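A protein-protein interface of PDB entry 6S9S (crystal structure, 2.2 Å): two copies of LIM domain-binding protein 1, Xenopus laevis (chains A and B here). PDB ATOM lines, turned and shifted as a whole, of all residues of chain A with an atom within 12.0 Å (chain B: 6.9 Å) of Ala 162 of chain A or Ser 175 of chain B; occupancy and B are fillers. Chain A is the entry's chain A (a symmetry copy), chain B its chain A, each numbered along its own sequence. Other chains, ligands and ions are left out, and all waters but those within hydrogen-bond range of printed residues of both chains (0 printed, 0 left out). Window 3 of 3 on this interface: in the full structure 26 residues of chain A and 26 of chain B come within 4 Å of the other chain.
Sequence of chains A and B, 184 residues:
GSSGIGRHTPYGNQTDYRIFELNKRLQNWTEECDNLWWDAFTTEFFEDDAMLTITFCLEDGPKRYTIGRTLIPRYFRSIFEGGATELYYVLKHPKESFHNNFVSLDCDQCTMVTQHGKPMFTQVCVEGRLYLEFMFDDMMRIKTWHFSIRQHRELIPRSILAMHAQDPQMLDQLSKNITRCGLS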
ATOM      1  N   PHE A 121     -10.209  28.592  -6.192  1.00  0.00           N
ATOM      2  CA  PHE A 121     -10.761  29.297  -7.372  1.00  0.00           C
ATOM      3  C   PHE A 121      -9.651  30.153  -8.005  1.00  0.00           C
ATOM      4  O   PHE A 121      -9.876  30.652  -9.127  1.00  0.00           O
ATOM      5  CB  PHE A 121     -12.012  30.106  -6.978  1.00  0.00           C
ATOM      6  CG  PHE A 121     -11.745  31.353  -6.173  1.00  0.00           C
ATOM      7  CD1 PHE A 121     -11.472  32.564  -6.793  1.00  0.00           C
ATOM      8  CD2 PHE A 121     -11.769  31.320  -4.783  1.00  0.00           C
ATOM      9  CE1 PHE A 121     -11.201  33.699  -6.033  1.00  0.00           C
ATOM     10  CE2 PHE A 121     -11.528  32.459  -4.024  1.00  0.00           C
ATOM     11  CZ  PHE A 121     -11.233  33.649  -4.649  1.00  0.00           C
ATOM     12  N   ILE A 156      -6.331  30.196 -12.796  1.00  0.00           N
ATOM     13  CA  ILE A 156      -7.713  29.802 -12.385  1.00  0.00           C
ATOM     14  C   ILE A 156      -7.949  28.405 -12.909  1.00  0.00           C
ATOM     15  O   ILE A 156      -7.429  28.073 -13.954  1.00  0.00           O
ATOM     16  CB  ILE A 156      -8.765  30.789 -12.926  1.00  0.00           C
ATOM     17  CG1 ILE A 156      -8.631  30.945 -14.443  1.00  0.00           C
ATOM     18  CG2 ILE A 156      -8.635  32.121 -12.223  1.00  0.00           C
ATOM     19  CD1 ILE A 156      -9.841  31.549 -15.116  1.00  0.00           C
ATOM     20  N   PRO A 157      -8.781  27.576 -12.253  1.00  0.00           N
ATOM     21  CA  PRO A 157      -9.136  26.271 -12.796  1.00  0.00           C
ATOM     22  C   PRO A 157      -9.675  26.450 -14.215  1.00  0.00           C
ATOM     23  O   PRO A 157     -10.356  27.443 -14.468  1.00  0.00           O
ATOM     24  CB  PRO A 157     -10.220  25.746 -11.848  1.00  0.00           C
ATOM     25  CG  PRO A 157      -9.934  26.464 -10.560  1.00  0.00           C
ATOM     26  CD  PRO A 157      -9.448  27.838 -10.980  1.00  0.00           C
ATOM     27  N   ARG A 158      -9.313  25.513 -15.083  1.00  0.00           N
ATOM     28  CA  ARG A 158      -9.866  25.364 -16.452  1.00  0.00           C
ATOM     29  C   ARG A 158     -11.386  25.176 -16.338  1.00  0.00           C
ATOM     30  O   ARG A 158     -12.107  25.605 -17.267  1.00  0.00           O
ATOM     31  CB  ARG A 158      -9.204  24.158 -17.126  1.00  0.00           C
ATOM     32  CG  ARG A 158      -9.166  24.199 -18.645  1.00  0.00           C
ATOM     33  CD  ARG A 158      -8.549  22.947 -19.253  1.00  0.00           C
ATOM     34  NE  ARG A 158      -7.089  22.937 -19.320  1.00  0.00           N
ATOM     35  CZ  ARG A 158      -6.342  23.770 -20.056  1.00  0.00           C
ATOM     36  NH1 ARG A 158      -6.910  24.730 -20.770  1.00  0.00           N
ATOM     37  NH2 ARG A 158      -5.022  23.665 -20.048  1.00  0.00           N
ATOM     38  N   SER A 159     -11.848  24.518 -15.267  1.00  0.00           N
ATOM     39  CA  SER A 159     -13.289  24.218 -15.045  1.00  0.00           C
ATOM     40  C   SER A 159     -14.112  25.521 -15.048  1.00  0.00           C
ATOM     41  O   SER A 159     -15.239  25.569 -15.669  1.00  0.00           O
ATOM     42  CB  SER A 159     -13.496  23.406 -13.805  1.00  0.00           C
ATOM     43  OG  SER A 159     -12.852  24.009 -12.681  1.00  0.00           O
ATOM     44  N   ILE A 160     -13.604  26.579 -14.379  1.00  0.00           N
ATOM     45  CA  ILE A 160     -14.292  27.904 -14.221  1.00  0.00           C
ATOM     46  C   ILE A 160     -14.525  28.487 -15.614  1.00  0.00           C
ATOM     47  O   ILE A 160     -15.555  29.161 -15.843  1.00  0.00           O
ATOM     48  CB  ILE A 160     -13.527  28.906 -13.318  1.00  0.00           C
ATOM     49  CG1 ILE A 160     -13.026  28.278 -12.008  1.00  0.00           C
ATOM     50  CG2 ILE A 160     -14.386  30.144 -13.038  1.00  0.00           C
ATOM     51  CD1 ILE A 160     -14.058  27.471 -11.240  1.00  0.00           C
ATOM     52  N   LEU A 161     -13.605  28.236 -16.528  1.00  0.00           N
ATOM     53  CA  LEU A 161     -13.721  28.778 -17.902  1.00  0.00           C
ATOM     54  C   LEU A 161     -14.803  28.013 -18.686  1.00  0.00           C
ATOM     55  O   LEU A 161     -15.665  28.675 -19.312  1.00  0.00           O
ATOM     56  CB  LEU A 161     -12.344  28.699 -18.559  1.00  0.00           C
ATOM     57  CG  LEU A 161     -12.253  29.372 -19.913  1.00  0.00           C
ATOM     58  CD1 LEU A 161     -10.849  29.918 -20.142  1.00  0.00           C
ATOM     59  CD2 LEU A 161     -12.627  28.378 -20.996  1.00  0.00           C
ATOM     60  N   ALA A 162     -14.791  26.676 -18.648  1.00  0.00           N
ATOM     61  CA  ALA A 162     -15.891  25.819 -19.166  1.00  0.00           C
ATOM     62  C   ALA A 162     -17.249  26.383 -18.701  1.00  0.00           C
ATOM     63  O   ALA A 162     -18.125  26.610 -19.548  1.00  0.00           O
ATOM     64  CB  ALA A 162     -15.706  24.392 -18.695  1.00  0.00           C
ATOM     65  N   MET A 163     -17.375  26.620 -17.386  1.00  0.00           N
ATOM     66  CA  MET A 163     -18.628  27.010 -16.698  1.00  0.00           C
ATOM     67  C   MET A 163     -19.233  28.260 -17.354  1.00  0.00           C
ATOM     68  O   MET A 163     -20.498  28.264 -17.598  1.00  0.00           O
ATOM     69  CB  MET A 163     -18.354  27.330 -15.227  1.00  0.00           C
ATOM     70  CG  MET A 163     -19.598  27.795 -14.489  1.00  0.00           C
ATOM     71  SD  MET A 163     -20.575  26.365 -13.991  1.00  0.00           S
ATOM     72  CE  MET A 163     -19.703  25.999 -12.462  1.00  0.00           C
ATOM     73  N   HIS A 164     -18.393  29.289 -17.571  1.00  0.00           N
ATOM     74  CA  HIS A 164     -18.830  30.672 -17.902  1.00  0.00           C
ATOM     75  C   HIS A 164     -18.458  31.013 -19.347  1.00  0.00           C
ATOM     76  O   HIS A 164     -18.347  32.191 -19.632  1.00  0.00           O
ATOM     77  CB  HIS A 164     -18.253  31.690 -16.899  1.00  0.00           C
ATOM     78  CG  HIS A 164     -18.745  31.525 -15.500  1.00  0.00           C
ATOM     79  ND1 HIS A 164     -20.091  31.531 -15.180  1.00  0.00           N
ATOM     80  CD2 HIS A 164     -18.085  31.409 -14.327  1.00  0.00           C
ATOM     81  CE1 HIS A 164     -20.230  31.367 -13.884  1.00  0.00           C
ATOM     82  NE2 HIS A 164     -19.020  31.315 -13.335  1.00  0.00           N
ATOM     83  N   ALA A 165     -18.266  30.003 -20.202  1.00  0.00           N
ATOM     84  CA  ALA A 165     -17.979  30.097 -21.668  1.00  0.00           C
ATOM     85  C   ALA A 165     -18.864  31.156 -22.343  1.00  0.00           C
ATOM     86  O   ALA A 165     -18.357  31.962 -23.139  1.00  0.00           O
ATOM     87  CB  ALA A 165     -18.237  28.756 -22.291  1.00  0.00           C
ATOM     88  N   GLN A 166     -20.143  31.173 -21.973  1.00  0.00           N
ATOM     89  CA  GLN A 166     -21.240  31.849 -22.709  1.00  0.00           C
ATOM     90  C   GLN A 166     -21.734  33.077 -21.939  1.00  0.00           C
ATOM     91  O   GLN A 166     -22.869  33.478 -22.184  1.00  0.00           O
ATOM     92  CB  GLN A 166     -22.350  30.820 -22.941  1.00  0.00           C
ATOM     93  CG  GLN A 166     -21.798  29.500 -23.480  1.00  0.00           C
ATOM     94  CD  GLN A 166     -22.430  29.033 -24.769  1.00  0.00           C
ATOM     95  OE1 GLN A 166     -23.640  29.159 -24.981  1.00  0.00           O
ATOM     96  NE2 GLN A 166     -21.601  28.474 -25.635  1.00  0.00           N
ATOM     97  N   ASP A 167     -20.898  33.656 -21.076  1.00  0.00           N
ATOM     98  CA  ASP A 167     -21.248  34.781 -20.161  1.00  0.00           C
ATOM     99  C   ASP A 167     -20.180  35.864 -20.343  1.00  0.00           C
ATOM    100  O   ASP A 167     -19.167  35.907 -19.584  1.00  0.00           O
ATOM    101  CB  ASP A 167     -21.361  34.274 -18.721  1.00  0.00           C
ATOM    102  CG  ASP A 167     -22.096  35.199 -17.764  1.00  0.00           C
ATOM    103  OD1 ASP A 167     -21.955  36.436 -17.913  1.00  0.00           O
ATOM    104  OD2 ASP A 167     -22.805  34.663 -16.860  1.00  0.00           O
ATOM    105  N   PRO A 168     -20.313  36.744 -21.368  1.00  0.00           N
ATOM    106  CA  PRO A 168     -19.297  37.764 -21.630  1.00  0.00           C
ATOM    107  C   PRO A 168     -18.979  38.559 -20.365  1.00  0.00           C
ATOM    108  O   PRO A 168     -17.829  38.792 -20.093  1.00  0.00           O
ATOM    109  CB  PRO A 168     -19.947  38.665 -22.685  1.00  0.00           C
ATOM    110  CG  PRO A 168     -20.868  37.708 -23.419  1.00  0.00           C
ATOM    111  CD  PRO A 168     -21.421  36.800 -22.338  1.00  0.00           C
ATOM    112  N   MET A 170     -19.430  37.733 -17.073  1.00  0.00           N
ATOM    113  CA  MET A 170     -18.709  36.925 -16.051  1.00  0.00           C
ATOM    114  C   MET A 170     -17.262  36.645 -16.508  1.00  0.00           C
ATOM    115  O   MET A 170     -16.357  36.584 -15.634  1.00  0.00           O
ATOM    116  CB  MET A 170     -19.441  35.615 -15.759  1.00  0.00           C
ATOM    117  CG  MET A 170     -18.830  34.827 -14.611  1.00  0.00           C
ATOM    118  SD  MET A 170     -18.917  35.647 -12.970  1.00  0.00           S
ATOM    119  CE  MET A 170     -18.193  34.384 -11.922  1.00  0.00           C
ATOM    120  N   LEU A 171     -17.026  36.489 -17.818  1.00  0.00           N
ATOM    121  CA  LEU A 171     -15.656  36.313 -18.362  1.00  0.00           C
ATOM    122  C   LEU A 171     -14.902  37.638 -18.229  1.00  0.00           C
ATOM    123  O   LEU A 171     -13.676  37.584 -18.056  1.00  0.00           O
ATOM    124  CB  LEU A 171     -15.716  35.842 -19.817  1.00  0.00           C
ATOM    125  CG  LEU A 171     -16.205  34.412 -20.023  1.00  0.00           C
ATOM    126  CD1 LEU A 171     -16.557  34.156 -21.478  1.00  0.00           C
ATOM    127  CD2 LEU A 171     -15.172  33.411 -19.545  1.00  0.00           C
ATOM    128  N   LEU A 174     -13.788  37.633 -14.582  1.00  0.00           N
ATOM    129  CA  LEU A 174     -12.777  36.573 -14.316  1.00  0.00           C
ATOM    130  C   LEU A 174     -11.407  36.987 -14.899  1.00  0.00           C
ATOM    131  O   LEU A 174     -10.372  36.503 -14.387  1.00  0.00           O
ATOM    132  CB  LEU A 174     -13.270  35.249 -14.904  1.00  0.00           C
ATOM    133  CG  LEU A 174     -14.328  34.529 -14.077  1.00  0.00           C
ATOM    134  CD1 LEU A 174     -14.962  33.411 -14.889  1.00  0.00           C
ATOM    135  CD2 LEU A 174     -13.753  34.000 -12.773  1.00  0.00           C
ATOM    136  N   ILE B 156      -4.838  27.767 -15.730  1.00  0.00           N
ATOM    137  CA  ILE B 156      -4.282  28.544 -16.879  1.00  0.00           C
ATOM    138  C   ILE B 156      -4.101  29.967 -16.404  1.00  0.00           C
ATOM    139  O   ILE B 156      -4.878  30.419 -15.589  1.00  0.00           O
ATOM    140  CB  ILE B 156      -5.210  28.477 -18.107  1.00  0.00           C
ATOM    141  CG1 ILE B 156      -6.629  28.918 -17.738  1.00  0.00           C
ATOM    142  CG2 ILE B 156      -5.201  27.081 -18.687  1.00  0.00           C
ATOM    143  CD1 ILE B 156      -7.496  29.278 -18.921  1.00  0.00           C
ATOM    144  N   MET B 170     -12.018  29.647 -29.571  1.00  0.00           N
ATOM    145  CA  MET B 170     -10.743  29.528 -28.810  1.00  0.00           C
ATOM    146  C   MET B 170     -11.030  29.269 -27.317  1.00  0.00           C
ATOM    147  O   MET B 170     -10.233  28.540 -26.670  1.00  0.00           O
ATOM    148  CB  MET B 170      -9.875  30.776 -28.981  1.00  0.00           C
ATOM    149  CG  MET B 170      -8.497  30.640 -28.352  1.00  0.00           C
ATOM    150  SD  MET B 170      -7.419  29.360 -29.107  1.00  0.00           S
ATOM    151  CE  MET B 170      -5.912  29.587 -28.162  1.00  0.00           C
ATOM    152  N   LEU B 171     -12.122  29.823 -26.771  1.00  0.00           N
ATOM    153  CA  LEU B 171     -12.533  29.554 -25.371  1.00  0.00           C
ATOM    154  C   LEU B 171     -13.031  28.110 -25.275  1.00  0.00           C
ATOM    155  O   LEU B 171     -12.861  27.515 -24.201  1.00  0.00           O
ATOM    156  CB  LEU B 171     -13.606  30.551 -24.928  1.00  0.00           C
ATOM    157  CG  LEU B 171     -13.126  31.985 -24.730  1.00  0.00           C
ATOM    158  CD1 LEU B 171     -14.297  32.948 -24.636  1.00  0.00           C
ATOM    159  CD2 LEU B 171     -12.248  32.099 -23.500  1.00  0.00           C
ATOM    160  N   ASP B 172     -13.595  27.552 -26.355  1.00  0.00           N
ATOM    161  CA  ASP B 172     -14.131  26.166 -26.330  1.00  0.00           C
ATOM    162  C   ASP B 172     -12.942  25.214 -26.213  1.00  0.00           C
ATOM    163  O   ASP B 172     -13.062  24.218 -25.474  1.00  0.00           O
ATOM    164  CB  ASP B 172     -15.032  25.822 -27.521  1.00  0.00           C
ATOM    165  CG  ASP B 172     -15.590  24.405 -27.407  1.00  0.00           C
ATOM    166  OD1 ASP B 172     -16.210  24.101 -26.324  1.00  0.00           O
ATOM    167  OD2 ASP B 172     -15.356  23.580 -28.366  1.00  0.00           O
ATOM    168  N   GLN B 173     -11.840  25.535 -26.898  1.00  0.00           N
ATOM    169  CA  GLN B 173     -10.597  24.712 -26.918  1.00  0.00           C
ATOM    170  C   GLN B 173      -9.846  24.884 -25.595  1.00  0.00           C
ATOM    171  O   GLN B 173      -9.276  23.886 -25.118  1.00  0.00           O
ATOM    172  CB  GLN B 173      -9.704  25.061 -28.114  1.00  0.00           C
ATOM    173  CG  GLN B 173     -10.035  24.259 -29.369  1.00  0.00           C
ATOM    174  CD  GLN B 173      -9.785  22.789 -29.128  1.00  0.00           C
ATOM    175  OE1 GLN B 173      -8.797  22.412 -28.474  1.00  0.00           O
ATOM    176  NE2 GLN B 173     -10.688  21.954 -29.635  1.00  0.00           N
ATOM    177  N   LEU B 174      -9.801  26.097 -25.041  1.00  0.00           N
ATOM    178  CA  LEU B 174      -9.083  26.355 -23.762  1.00  0.00           C
ATOM    179  C   LEU B 174      -9.801  25.637 -22.596  1.00  0.00           C
ATOM    180  O   LEU B 174      -9.130  25.329 -21.585  1.00  0.00           O
ATOM    181  CB  LEU B 174      -8.990  27.865 -23.532  1.00  0.00           C
ATOM    182  CG  LEU B 174      -7.918  28.577 -24.346  1.00  0.00           C
ATOM    183  CD1 LEU B 174      -8.118  30.083 -24.279  1.00  0.00           C
ATOM    184  CD2 LEU B 174      -6.521  28.191 -23.887  1.00  0.00           C
ATOM    185  N   SER B 175     -11.093  25.347 -22.770  1.00  0.00           N
ATOM    186  CA  SER B 175     -11.970  24.585 -21.843  1.00  0.00           C
ATOM    187  C   SER B 175     -11.487  23.157 -21.629  1.00  0.00           C
ATOM    188  O   SER B 175     -11.847  22.576 -20.580  1.00  0.00           O
ATOM    189  CB  SER B 175     -13.369  24.518 -22.364  1.00  0.00           C
ATOM    190  OG  SER B 175     -14.026  25.735 -22.074  1.00  0.00           O
ATOM    191  N   LYS B 176     -10.777  22.593 -22.607  1.00  0.00           N
ATOM    192  CA  LYS B 176     -10.522  21.134 -22.650  1.00  0.00           C
ATOM    193  C   LYS B 176      -9.211  20.889 -21.913  1.00  0.00           C
ATOM    194  O   LYS B 176      -8.257  21.658 -22.121  1.00  0.00           O
ATOM    195  CB  LYS B 176     -10.550  20.605 -24.090  1.00  0.00           C
ATOM    196  CG  LYS B 176     -11.585  21.275 -24.986  1.00  0.00           C
ATOM    197  CD  LYS B 176     -11.798  20.627 -26.353  1.00  0.00           C
ATOM    198  CE  LYS B 176     -12.990  19.691 -26.398  1.00  0.00           C
ATOM    199  NZ  LYS B 176     -12.973  18.884 -27.638  1.00  0.00           N
ATOM    200  N   ASN B 177      -9.206  19.888 -21.034  1.00  0.00           N
ATOM    201  CA  ASN B 177      -7.974  19.346 -20.415  1.00  0.00           C
ATOM    202  C   ASN B 177      -7.003  18.950 -21.541  1.00  0.00           C
ATOM    203  O   ASN B 177      -7.491  18.456 -22.586  1.00  0.00           O
ATOM    204  CB  ASN B 177      -8.334  18.218 -19.452  1.00  0.00           C
ATOM    205  CG  ASN B 177      -8.846  18.764 -18.133  1.00  0.00           C
ATOM    206  OD1 ASN B 177      -9.101  19.956 -17.998  1.00  0.00           O
ATOM    207  ND2 ASN B 177      -8.958  17.903 -17.139  1.00  0.00           N
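The backbone carbonyl oxygen (O) of Lys 176 of chain B lies close to the guanidinium group (NE) of Arg 158 of chain A (3.3 Å). O of Leu 174 of chain B is in hydrogen-bond range of NH1 of Arg 158 of chain A, 2.4 Å away. O of Ile 156 of chain A lies within hydrogen-bond range of N of Ile 156 of chain B (3.2 Å).
The side-chain hydroxyl of Ser 175 of chain B lies within hydrogen-bond range of the backbone carbonyl oxygen of Leu 171 of chain B.
Among the printed residues, pairs that only touch across the chains: Leu 161 of chain A with Ser 175 of chain B (3.2 Å), Arg 158 of chain A with Asn 177 of chain B (3.3 Å), Leu 161 of chain A with Leu 171 of chain B (3.3 Å), Ala 162 of chain A with Ser 175 of chain B (3.5 Å), Arg 158 of chain A with Ser 175 of chain B (3.6 Å), Arg 158 of chain A with Ile 156 of chain B (3.6 Å) and Leu 161 of chain A with Ile 156 of chain B (3.6 Å).
Phe 121 of chain A touches none of the printed residues of chain B. Printed residues of chain B within 4 Å of Ile 156 of chain A: Ile 156. Printed residues of chain B within 4 Å of Arg 158 of chain A: Ile 156 (3.6 Å), Leu 174 (2.4 Å), Ser 175 (3.6 Å), Lys 176 (3.2 Å) and Asn 177 (3.3 Å). Printed residues of chain B within 4 Å of Leu 161 of chain A: Ile 156, Leu 171 and Ser 175. Of the printed residues of chain B, Ala 162 of chain A touches Ser 175 (3.5 Å). Leu 174 of chain A touches none of the printed residues of chain B. Printed residues of chain A within 4 Å of Ile 156 of chain B: Ile 156 (3.2 Å), Arg 158 (3.6 Å) and Leu 161 (3.6 Å). Of chain A, only Leu 161 (3.3 Å) comes within 4 Å of Leu 171 of chain B. No residue of chain A comes within 4 Å of Asp 172 of chain B. No residue of chain A comes within 4 Å of Gln 173 of chain B. Leu 174 of chain B touches just one residue of chain A: Arg 158. Of chain A, only Arg 158, Leu 161 and Ala 162 come within 4 Å of Ser 175 of chain B. Of chain A, only Arg 158 (3.2 Å) comes within 4 Å of Lys 176 of chain B. Of chain A, only Arg 158 comes within 4 Å of Asn 177 of chain B. The nearest residue of chain B that does not touch Ala 162 of chain A is Leu 171 of chain B (5.9 Å). The nearest residue of chain A that does not touch Ser 175 of chain B is Ala 165 of chain A (5.2 Å).
Hydrophobic or aromatic side chains of chain B within 4 Å of the printed part of chain A: Ile 156. Printed residues of chain A that touch a printed residue of chain B: Ile 156, Arg 158, Leu 161 and Ala 162. Hydrophobic or aromatic side chains of chain A that line the printed part of chain B: Ile 156 and Leu 161. Among the printed residues, 10 pairs touch across the chains. Among the printed residues, no Asp or Glu carboxylate lies within 4 Å of a Lys or Arg side-chain nitrogen of the other chain.
Ile 156 of chain B touches its own counterpart, Ile 156 of chain A.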
